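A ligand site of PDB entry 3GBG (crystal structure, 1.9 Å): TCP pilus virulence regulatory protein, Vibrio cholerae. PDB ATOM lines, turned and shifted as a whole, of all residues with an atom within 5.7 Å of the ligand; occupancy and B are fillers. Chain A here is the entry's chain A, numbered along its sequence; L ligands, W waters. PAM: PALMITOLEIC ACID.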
ATOM      1  N   GLN A   8      17.789  15.194  30.702  1.00  0.00           N
ATOM      2  CA  GLN A   8      18.688  14.616  29.698  1.00  0.00           C
ATOM      3  C   GLN A   8      20.107  14.874  30.210  1.00  0.00           C
ATOM      4  O   GLN A   8      20.509  16.024  30.349  1.00  0.00           O
ATOM      5  CB  GLN A   8      18.459  15.318  28.350  1.00  0.00           C
ATOM      6  CG  GLN A   8      18.950  14.557  27.132  1.00  0.00           C
ATOM      7  CD  GLN A   8      20.459  14.527  27.040  1.00  0.00           C
ATOM      8  OE1 GLN A   8      21.083  13.475  27.103  1.00  0.00           O
ATOM      9  NE2 GLN A   8      21.056  15.698  26.851  1.00  0.00           N
ATOM     10  N   ASN A  10      24.499  14.050  30.255  1.00  0.00           N
ATOM     11  CA  ASN A  10      25.693  13.582  29.560  1.00  0.00           C
ATOM     12  C   ASN A  10      26.905  13.802  30.453  1.00  0.00           C
ATOM     13  O   ASN A  10      26.901  14.679  31.325  1.00  0.00           O
ATOM     14  CB  ASN A  10      25.878  14.351  28.248  1.00  0.00           C
ATOM     15  CG  ASN A  10      24.732  14.156  27.291  1.00  0.00           C
ATOM     16  OD1 ASN A  10      23.782  14.946  27.279  1.00  0.00           O
ATOM     17  ND2 ASN A  10      24.805  13.109  26.490  1.00  0.00           N
ATOM     18  N   TYR A  12      31.126  14.269  30.234  1.00  0.00           N
ATOM     19  CA  TYR A  12      32.264  14.520  29.362  1.00  0.00           C
ATOM     20  C   TYR A  12      33.580  14.426  30.118  1.00  0.00           C
ATOM     21  O   TYR A  12      33.721  14.943  31.222  1.00  0.00           O
ATOM     22  CB  TYR A  12      32.161  15.912  28.728  1.00  0.00           C
ATOM     23  CG  TYR A  12      30.885  16.151  27.948  1.00  0.00           C
ATOM     24  CD1 TYR A  12      29.787  16.770  28.535  1.00  0.00           C
ATOM     25  CD2 TYR A  12      30.773  15.726  26.636  1.00  0.00           C
ATOM     26  CE1 TYR A  12      28.604  16.978  27.826  1.00  0.00           C
ATOM     27  CE2 TYR A  12      29.604  15.920  25.913  1.00  0.00           C
ATOM     28  CZ  TYR A  12      28.520  16.546  26.508  1.00  0.00           C
ATOM     29  OH  TYR A  12      27.360  16.717  25.802  1.00  0.00           O
ATOM     30  N   TYR A  20      38.149  23.860  27.578  1.00  0.00           N
ATOM     31  CA  TYR A  20      37.032  23.803  26.650  1.00  0.00           C
ATOM     32  C   TYR A  20      36.654  25.266  26.447  1.00  0.00           C
ATOM     33  O   TYR A  20      36.580  26.028  27.411  1.00  0.00           O
ATOM     34  CB  TYR A  20      35.873  23.007  27.261  1.00  0.00           C
ATOM     35  CG  TYR A  20      36.079  21.508  27.203  1.00  0.00           C
ATOM     36  CD1 TYR A  20      35.575  20.676  28.193  1.00  0.00           C
ATOM     37  CD2 TYR A  20      36.800  20.931  26.156  1.00  0.00           C
ATOM     38  CE1 TYR A  20      35.780  19.291  28.150  1.00  0.00           C
ATOM     39  CE2 TYR A  20      37.003  19.556  26.094  1.00  0.00           C
ATOM     40  CZ  TYR A  20      36.496  18.746  27.095  1.00  0.00           C
ATOM     41  OH  TYR A  20      36.714  17.388  27.030  1.00  0.00           O
ATOM     42  N   PHE A  22      33.847  27.948  24.580  1.00  0.00           N
ATOM     43  CA  PHE A  22      32.564  28.098  23.911  1.00  0.00           C
ATOM     44  C   PHE A  22      32.361  29.537  23.484  1.00  0.00           C
ATOM     45  O   PHE A  22      32.581  30.463  24.269  1.00  0.00           O
ATOM     46  CB  PHE A  22      31.448  27.657  24.852  1.00  0.00           C
ATOM     47  CG  PHE A  22      31.602  26.251  25.352  1.00  0.00           C
ATOM     48  CD1 PHE A  22      31.256  25.180  24.538  1.00  0.00           C
ATOM     49  CD2 PHE A  22      32.154  25.985  26.595  1.00  0.00           C
ATOM     50  CE1 PHE A  22      31.452  23.855  24.950  1.00  0.00           C
ATOM     51  CE2 PHE A  22      32.365  24.667  27.024  1.00  0.00           C
ATOM     52  CZ  PHE A  22      32.011  23.608  26.202  1.00  0.00           C
ATOM     53  N   LEU A  25      27.494  30.207  22.144  1.00  0.00           N
ATOM     54  CA  LEU A  25      26.807  28.955  22.391  1.00  0.00           C
ATOM     55  C   LEU A  25      25.378  29.229  22.863  1.00  0.00           C
ATOM     56  O   LEU A  25      25.168  29.727  23.971  1.00  0.00           O
ATOM     57  CB  LEU A  25      27.546  28.149  23.451  1.00  0.00           C
ATOM     58  CG  LEU A  25      26.926  26.812  23.854  1.00  0.00           C
ATOM     59  CD1 LEU A  25      27.037  25.832  22.679  1.00  0.00           C
ATOM     60  CD2 LEU A  25      27.645  26.259  25.071  1.00  0.00           C
ATOM     61  N   ILE A  27      21.818  28.358  24.348  1.00  0.00           N
ATOM     62  CA  ILE A  27      21.280  27.368  25.258  1.00  0.00           C
ATOM     63  C   ILE A  27      19.805  27.075  24.911  1.00  0.00           C
ATOM     64  O   ILE A  27      18.910  27.857  25.245  1.00  0.00           O
ATOM     65  CB  ILE A  27      21.388  27.848  26.726  1.00  0.00           C
ATOM     66  CG1 ILE A  27      22.807  28.389  26.981  1.00  0.00           C
ATOM     67  CG2 ILE A  27      21.087  26.710  27.681  1.00  0.00           C
ATOM     68  CD1 ILE A  27      23.931  27.360  26.804  1.00  0.00           C
ATOM     69  N   LYS A  31      20.099  24.350  31.475  1.00  0.00           N
ATOM     70  CA  LYS A  31      21.134  23.348  31.717  1.00  0.00           C
ATOM     71  C   LYS A  31      21.915  23.655  32.992  1.00  0.00           C
ATOM     72  O   LYS A  31      21.925  24.780  33.471  1.00  0.00           O
ATOM     73  CB  LYS A  31      22.126  23.322  30.539  1.00  0.00           C
ATOM     74  CG  LYS A  31      21.561  22.809  29.230  1.00  0.00           C
ATOM     75  CD  LYS A  31      22.607  22.935  28.128  1.00  0.00           C
ATOM     76  CE  LYS A  31      22.119  22.352  26.810  1.00  0.00           C
ATOM     77  NZ  LYS A  31      22.027  20.864  26.868  1.00  0.00           N
ATOM     78  N   PHE A  33      25.699  22.183  35.008  1.00  0.00           N
ATOM     79  CA  PHE A  33      26.831  21.287  34.957  1.00  0.00           C
ATOM     80  C   PHE A  33      27.757  21.497  36.136  1.00  0.00           C
ATOM     81  O   PHE A  33      27.679  22.502  36.824  1.00  0.00           O
ATOM     82  CB  PHE A  33      27.622  21.461  33.656  1.00  0.00           C
ATOM     83  CG  PHE A  33      28.325  22.793  33.531  1.00  0.00           C
ATOM     84  CD1 PHE A  33      27.683  23.881  32.931  1.00  0.00           C
ATOM     85  CD2 PHE A  33      29.630  22.943  33.982  1.00  0.00           C
ATOM     86  CE1 PHE A  33      28.342  25.100  32.782  1.00  0.00           C
ATOM     87  CE2 PHE A  33      30.301  24.159  33.840  1.00  0.00           C
ATOM     88  CZ  PHE A  33      29.657  25.248  33.230  1.00  0.00           C
ATOM     89  N   LEU A  61      22.862  27.414  33.374  1.00  0.00           N
ATOM     90  CA  LEU A  61      22.814  28.167  32.121  1.00  0.00           C
ATOM     91  C   LEU A  61      21.345  28.459  31.784  1.00  0.00           C
ATOM     92  O   LEU A  61      20.532  27.539  31.680  1.00  0.00           O
ATOM     93  CB  LEU A  61      23.477  27.366  31.007  1.00  0.00           C
ATOM     94  CG  LEU A  61      24.933  26.954  31.323  1.00  0.00           C
ATOM     95  CD1 LEU A  61      25.526  26.169  30.163  1.00  0.00           C
ATOM     96  CD2 LEU A  61      25.767  28.200  31.597  1.00  0.00           C
ATOM     97  N   PHE A  69      32.253  31.500  27.182  1.00  0.00           N
ATOM     98  CA  PHE A  69      33.117  31.179  28.325  1.00  0.00           C
ATOM     99  C   PHE A  69      34.005  29.978  28.079  1.00  0.00           C
ATOM    100  O   PHE A  69      33.819  29.236  27.110  1.00  0.00           O
ATOM    101  CB  PHE A  69      32.266  30.905  29.563  1.00  0.00           C
ATOM    102  CG  PHE A  69      31.497  29.607  29.498  1.00  0.00           C
ATOM    103  CD1 PHE A  69      30.316  29.516  28.788  1.00  0.00           C
ATOM    104  CD2 PHE A  69      31.978  28.464  30.142  1.00  0.00           C
ATOM    105  CE1 PHE A  69      29.611  28.315  28.713  1.00  0.00           C
ATOM    106  CE2 PHE A  69      31.275  27.263  30.076  1.00  0.00           C
ATOM    107  CZ  PHE A  69      30.084  27.185  29.358  1.00  0.00           C
ATOM    108  N   LEU A  71      36.342  26.713  30.211  1.00  0.00           N
ATOM    109  CA  LEU A  71      36.511  25.930  31.425  1.00  0.00           C
ATOM    110  C   LEU A  71      37.881  25.265  31.300  1.00  0.00           C
ATOM    111  O   LEU A  71      38.134  24.533  30.349  1.00  0.00           O
ATOM    112  CB  LEU A  71      35.425  24.853  31.539  1.00  0.00           C
ATOM    113  CG  LEU A  71      35.324  24.137  32.887  1.00  0.00           C
ATOM    114  CD1 LEU A  71      34.914  25.144  33.964  1.00  0.00           C
ATOM    115  CD2 LEU A  71      34.315  22.997  32.797  1.00  0.00           C
ATOM    116  N   VAL A  81      32.851  15.967  33.659  1.00  0.00           N
ATOM    117  CA  VAL A  81      31.907  17.065  33.718  1.00  0.00           C
ATOM    118  C   VAL A  81      30.534  16.502  33.411  1.00  0.00           C
ATOM    119  O   VAL A  81      30.326  15.929  32.350  1.00  0.00           O
ATOM    120  CB  VAL A  81      32.273  18.155  32.685  1.00  0.00           C
ATOM    121  CG1 VAL A  81      31.331  19.347  32.839  1.00  0.00           C
ATOM    122  CG2 VAL A  81      33.716  18.597  32.870  1.00  0.00           C
ATOM    123  N   VAL A  83      26.574  17.038  32.689  1.00  0.00           N
ATOM    124  CA  VAL A  83      25.683  18.064  32.171  1.00  0.00           C
ATOM    125  C   VAL A  83      24.246  17.582  32.147  1.00  0.00           C
ATOM    126  O   VAL A  83      23.912  16.582  31.497  1.00  0.00           O
ATOM    127  CB  VAL A  83      26.094  18.510  30.757  1.00  0.00           C
ATOM    128  CG1 VAL A  83      25.205  19.660  30.305  1.00  0.00           C
ATOM    129  CG2 VAL A  83      27.560  18.934  30.742  1.00  0.00           C
ATOM    130  N   THR A  85      20.317  18.436  31.225  1.00  0.00           N
ATOM    131  CA  THR A  85      19.448  19.288  30.430  1.00  0.00           C
ATOM    132  C   THR A  85      18.018  19.027  30.903  1.00  0.00           C
ATOM    133  O   THR A  85      17.562  17.892  30.930  1.00  0.00           O
ATOM    134  CB  THR A  85      19.602  18.962  28.931  1.00  0.00           C
ATOM    135  OG1 THR A  85      20.982  19.040  28.574  1.00  0.00           O
ATOM    136  CG2 THR A  85      18.822  19.956  28.101  1.00  0.00           C
ATOM    137  N   ILE A 226      23.515  19.565  17.921  1.00  0.00           N
ATOM    138  CA  ILE A 226      23.953  18.831  19.110  1.00  0.00           C
ATOM    139  C   ILE A 226      22.806  17.918  19.571  1.00  0.00           C
ATOM    140  O   ILE A 226      23.022  16.740  19.871  1.00  0.00           O
ATOM    141  CB  ILE A 226      24.365  19.799  20.234  1.00  0.00           C
ATOM    142  CG1 ILE A 226      25.674  20.480  19.853  1.00  0.00           C
ATOM    143  CG2 ILE A 226      24.516  19.054  21.566  1.00  0.00           C
ATOM    144  CD1 ILE A 226      26.026  21.674  20.751  1.00  0.00           C
ATOM    145  N   LYS A 230      22.680  13.759  19.899  1.00  0.00           N
ATOM    146  CA  LYS A 230      22.334  13.079  21.147  1.00  0.00           C
ATOM    147  C   LYS A 230      21.267  12.003  20.970  1.00  0.00           C
ATOM    148  O   LYS A 230      21.198  11.086  21.781  1.00  0.00           O
ATOM    149  CB  LYS A 230      21.856  14.102  22.188  1.00  0.00           C
ATOM    150  CG  LYS A 230      22.952  14.981  22.751  1.00  0.00           C
ATOM    151  CD  LYS A 230      22.447  15.797  23.943  1.00  0.00           C
ATOM    152  CE  LYS A 230      23.544  16.727  24.457  1.00  0.00           C
ATOM    153  NZ  LYS A 230      23.106  17.517  25.644  1.00  0.00           N
ATOM    154  N   MET A 259      32.034  25.411  19.414  1.00  0.00           N
ATOM    155  CA  MET A 259      32.419  24.390  20.389  1.00  0.00           C
ATOM    156  C   MET A 259      33.930  24.198  20.527  1.00  0.00           C
ATOM    157  O   MET A 259      34.381  23.457  21.406  1.00  0.00           O
ATOM    158  CB  MET A 259      31.798  23.051  19.994  1.00  0.00           C
ATOM    159  CG  MET A 259      30.284  23.089  19.872  1.00  0.00           C
ATOM    160  SD  MET A 259      29.453  23.310  21.462  1.00  0.00           S
ATOM    161  CE  MET A 259      29.561  21.670  22.106  1.00  0.00           C
ATOM    162  N   VAL A 261      35.721  22.474  18.818  1.00  0.00           N
ATOM    163  CA  VAL A 261      36.051  21.105  18.421  1.00  0.00           C
ATOM    164  C   VAL A 261      35.253  20.812  17.150  1.00  0.00           C
ATOM    165  O   VAL A 261      34.297  21.517  16.829  1.00  0.00           O
ATOM    166  CB  VAL A 261      35.654  20.064  19.503  1.00  0.00           C
ATOM    167  CG1 VAL A 261      36.376  20.355  20.812  1.00  0.00           C
ATOM    168  CG2 VAL A 261      34.140  20.077  19.729  1.00  0.00           C
ATOM    169  N   TYR A 266      33.025  15.998  18.707  1.00  0.00           N
ATOM    170  CA  TYR A 266      32.031  16.085  19.764  1.00  0.00           C
ATOM    171  C   TYR A 266      31.188  14.806  19.818  1.00  0.00           C
ATOM    172  O   TYR A 266      30.933  14.266  20.898  1.00  0.00           O
ATOM    173  CB  TYR A 266      31.107  17.298  19.557  1.00  0.00           C
ATOM    174  CG  TYR A 266      29.948  17.309  20.524  1.00  0.00           C
ATOM    175  CD1 TYR A 266      28.676  16.896  20.129  1.00  0.00           C
ATOM    176  CD2 TYR A 266      30.124  17.678  21.851  1.00  0.00           C
ATOM    177  CE1 TYR A 266      27.613  16.842  21.032  1.00  0.00           C
ATOM    178  CE2 TYR A 266      29.085  17.620  22.769  1.00  0.00           C
ATOM    179  CZ  TYR A 266      27.832  17.211  22.360  1.00  0.00           C
ATOM    180  OH  TYR A 266      26.816  17.127  23.273  1.00  0.00           O
ATOM    181  N   MET A 269      32.707  12.224  21.700  1.00  0.00           N
ATOM    182  CA  MET A 269      32.657  12.473  23.133  1.00  0.00           C
ATOM    183  C   MET A 269      31.329  12.005  23.720  1.00  0.00           C
ATOM    184  O   MET A 269      31.195  11.849  24.931  1.00  0.00           O
ATOM    185  CB  MET A 269      32.848  13.963  23.421  1.00  0.00           C
ATOM    186  CG  MET A 269      34.097  14.552  22.774  1.00  0.00           C
ATOM    187  SD  MET A 269      34.378  16.271  23.266  1.00  0.00           S
ATOM    188  CE  MET A 269      35.924  16.114  24.176  1.00  0.00           C
HETATM  189  C1  PAM L   1      25.679  19.798  25.805  1.00  0.00           C
HETATM  190  O1  PAM L   1      25.823  18.725  26.421  1.00  0.00           O
HETATM  191  O2  PAM L   1      24.532  20.263  25.681  1.00  0.00           O
HETATM  192  C2  PAM L   1      26.879  20.522  25.214  1.00  0.00           C
HETATM  193  C3  PAM L   1      26.850  22.005  25.611  1.00  0.00           C
HETATM  194  C4  PAM L   1      28.045  22.352  26.482  1.00  0.00           C
HETATM  195  C5  PAM L   1      27.626  23.240  27.648  1.00  0.00           C
HETATM  196  C6  PAM L   1      27.952  22.556  28.987  1.00  0.00           C
HETATM  197  C7  PAM L   1      29.205  23.152  29.618  1.00  0.00           C
HETATM  198  C8  PAM L   1      30.031  22.083  30.312  1.00  0.00           C
HETATM  199  C9  PAM L   1      31.524  22.249  29.985  1.00  0.00           C
HETATM  200  C10 PAM L   1      32.236  21.321  29.368  1.00  0.00           C
HETATM  201  C11 PAM L   1      31.625  19.979  28.929  1.00  0.00           C
HETATM  202  C12 PAM L   1      31.177  20.011  27.461  1.00  0.00           C
HETATM  203  C13 PAM L   1      32.304  19.617  26.527  1.00  0.00           C
HETATM  204  C14 PAM L   1      31.908  19.853  25.076  1.00  0.00           C
HETATM  205  C15 PAM L   1      33.040  19.469  24.152  1.00  0.00           C
HETATM  206  C16 PAM L   1      33.779  20.704  23.637  1.00  0.00           C
HETATM  207  O   HOH W   1      36.075  23.100  23.658  1.00  0.00           O
HETATM  208  O   HOH W   2      23.735  22.249  23.529  1.00  0.00           O
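The side-chain hydroxyl of Tyr 12 lies within hydrogen-bond range of an oxygen (O1) of the ligand (2.6 Å). The side-chain amino group (NZ) of Lys 31 is in salt-bridge range of an oxygen (O2) of the ligand (2.8 Å). The side-chain amino group of Lys 230 lies within salt-bridge range of an oxygen (O1) of the ligand (3.1 Å).
The side-chain hydroxyl (OH) of Tyr 12 sits at hydrogen-bond distance from the side-chain hydroxyl (OH) of Tyr 266, 2.6 Å away. O of Tyr 12 sits at hydrogen-bond distance from N of Val 81, 2.8 Å away. The backbone carbonyl oxygen of Lys 31 is in hydrogen-bond range of the backbone NH of Leu 61, 2.8 Å away. The side-chain hydroxyl (OG1) of Thr 85 lies within hydrogen-bond range of the side-chain amino group (NZ) of Lys 31, 2.7 Å away. OD1 of Asn 10 is in hydrogen-bond range of NZ of Lys 230, 3.1 Å away. NZ of Lys 230 sits close to NE2 of Gln 8 (3.0 Å). N of Tyr 20 is in hydrogen-bond range of O of Leu 71, at 2.9 Å. N of Phe 22 sits at hydrogen-bond distance from O of Phe 69 (2.8 Å).
CD1 of Tyr 20 touches C10 of the ligand, 3.6 Å away. Phe 22 touches the ligand (CZ to C12, 3.9 Å). Leu 25 touches the ligand (CD2 to C5, 3.97 Å). Phe 33 touches the ligand (CG to C8, 3.7 Å). Val 81 touches the ligand. Met 259 touches the ligand (O to C16, 3.6 Å). Val 261 touches the ligand. OH of Tyr 266 touches O1 of the ligand, at 3.7 Å. Met 269 touches the ligand. Hydrophobic or aromatic side chains that line the ligand: Tyr 12, Tyr 20, Phe 22, Leu 25, Phe 33, Val 81, Val 261 and Met 269. Within 4 Å of the ligand: Tyr 12, Tyr 20, Phe 22, Leu 25, Lys 31, Phe 33, Val 81, Lys 230, Met 259, Val 261, Tyr 266 and Met 269.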
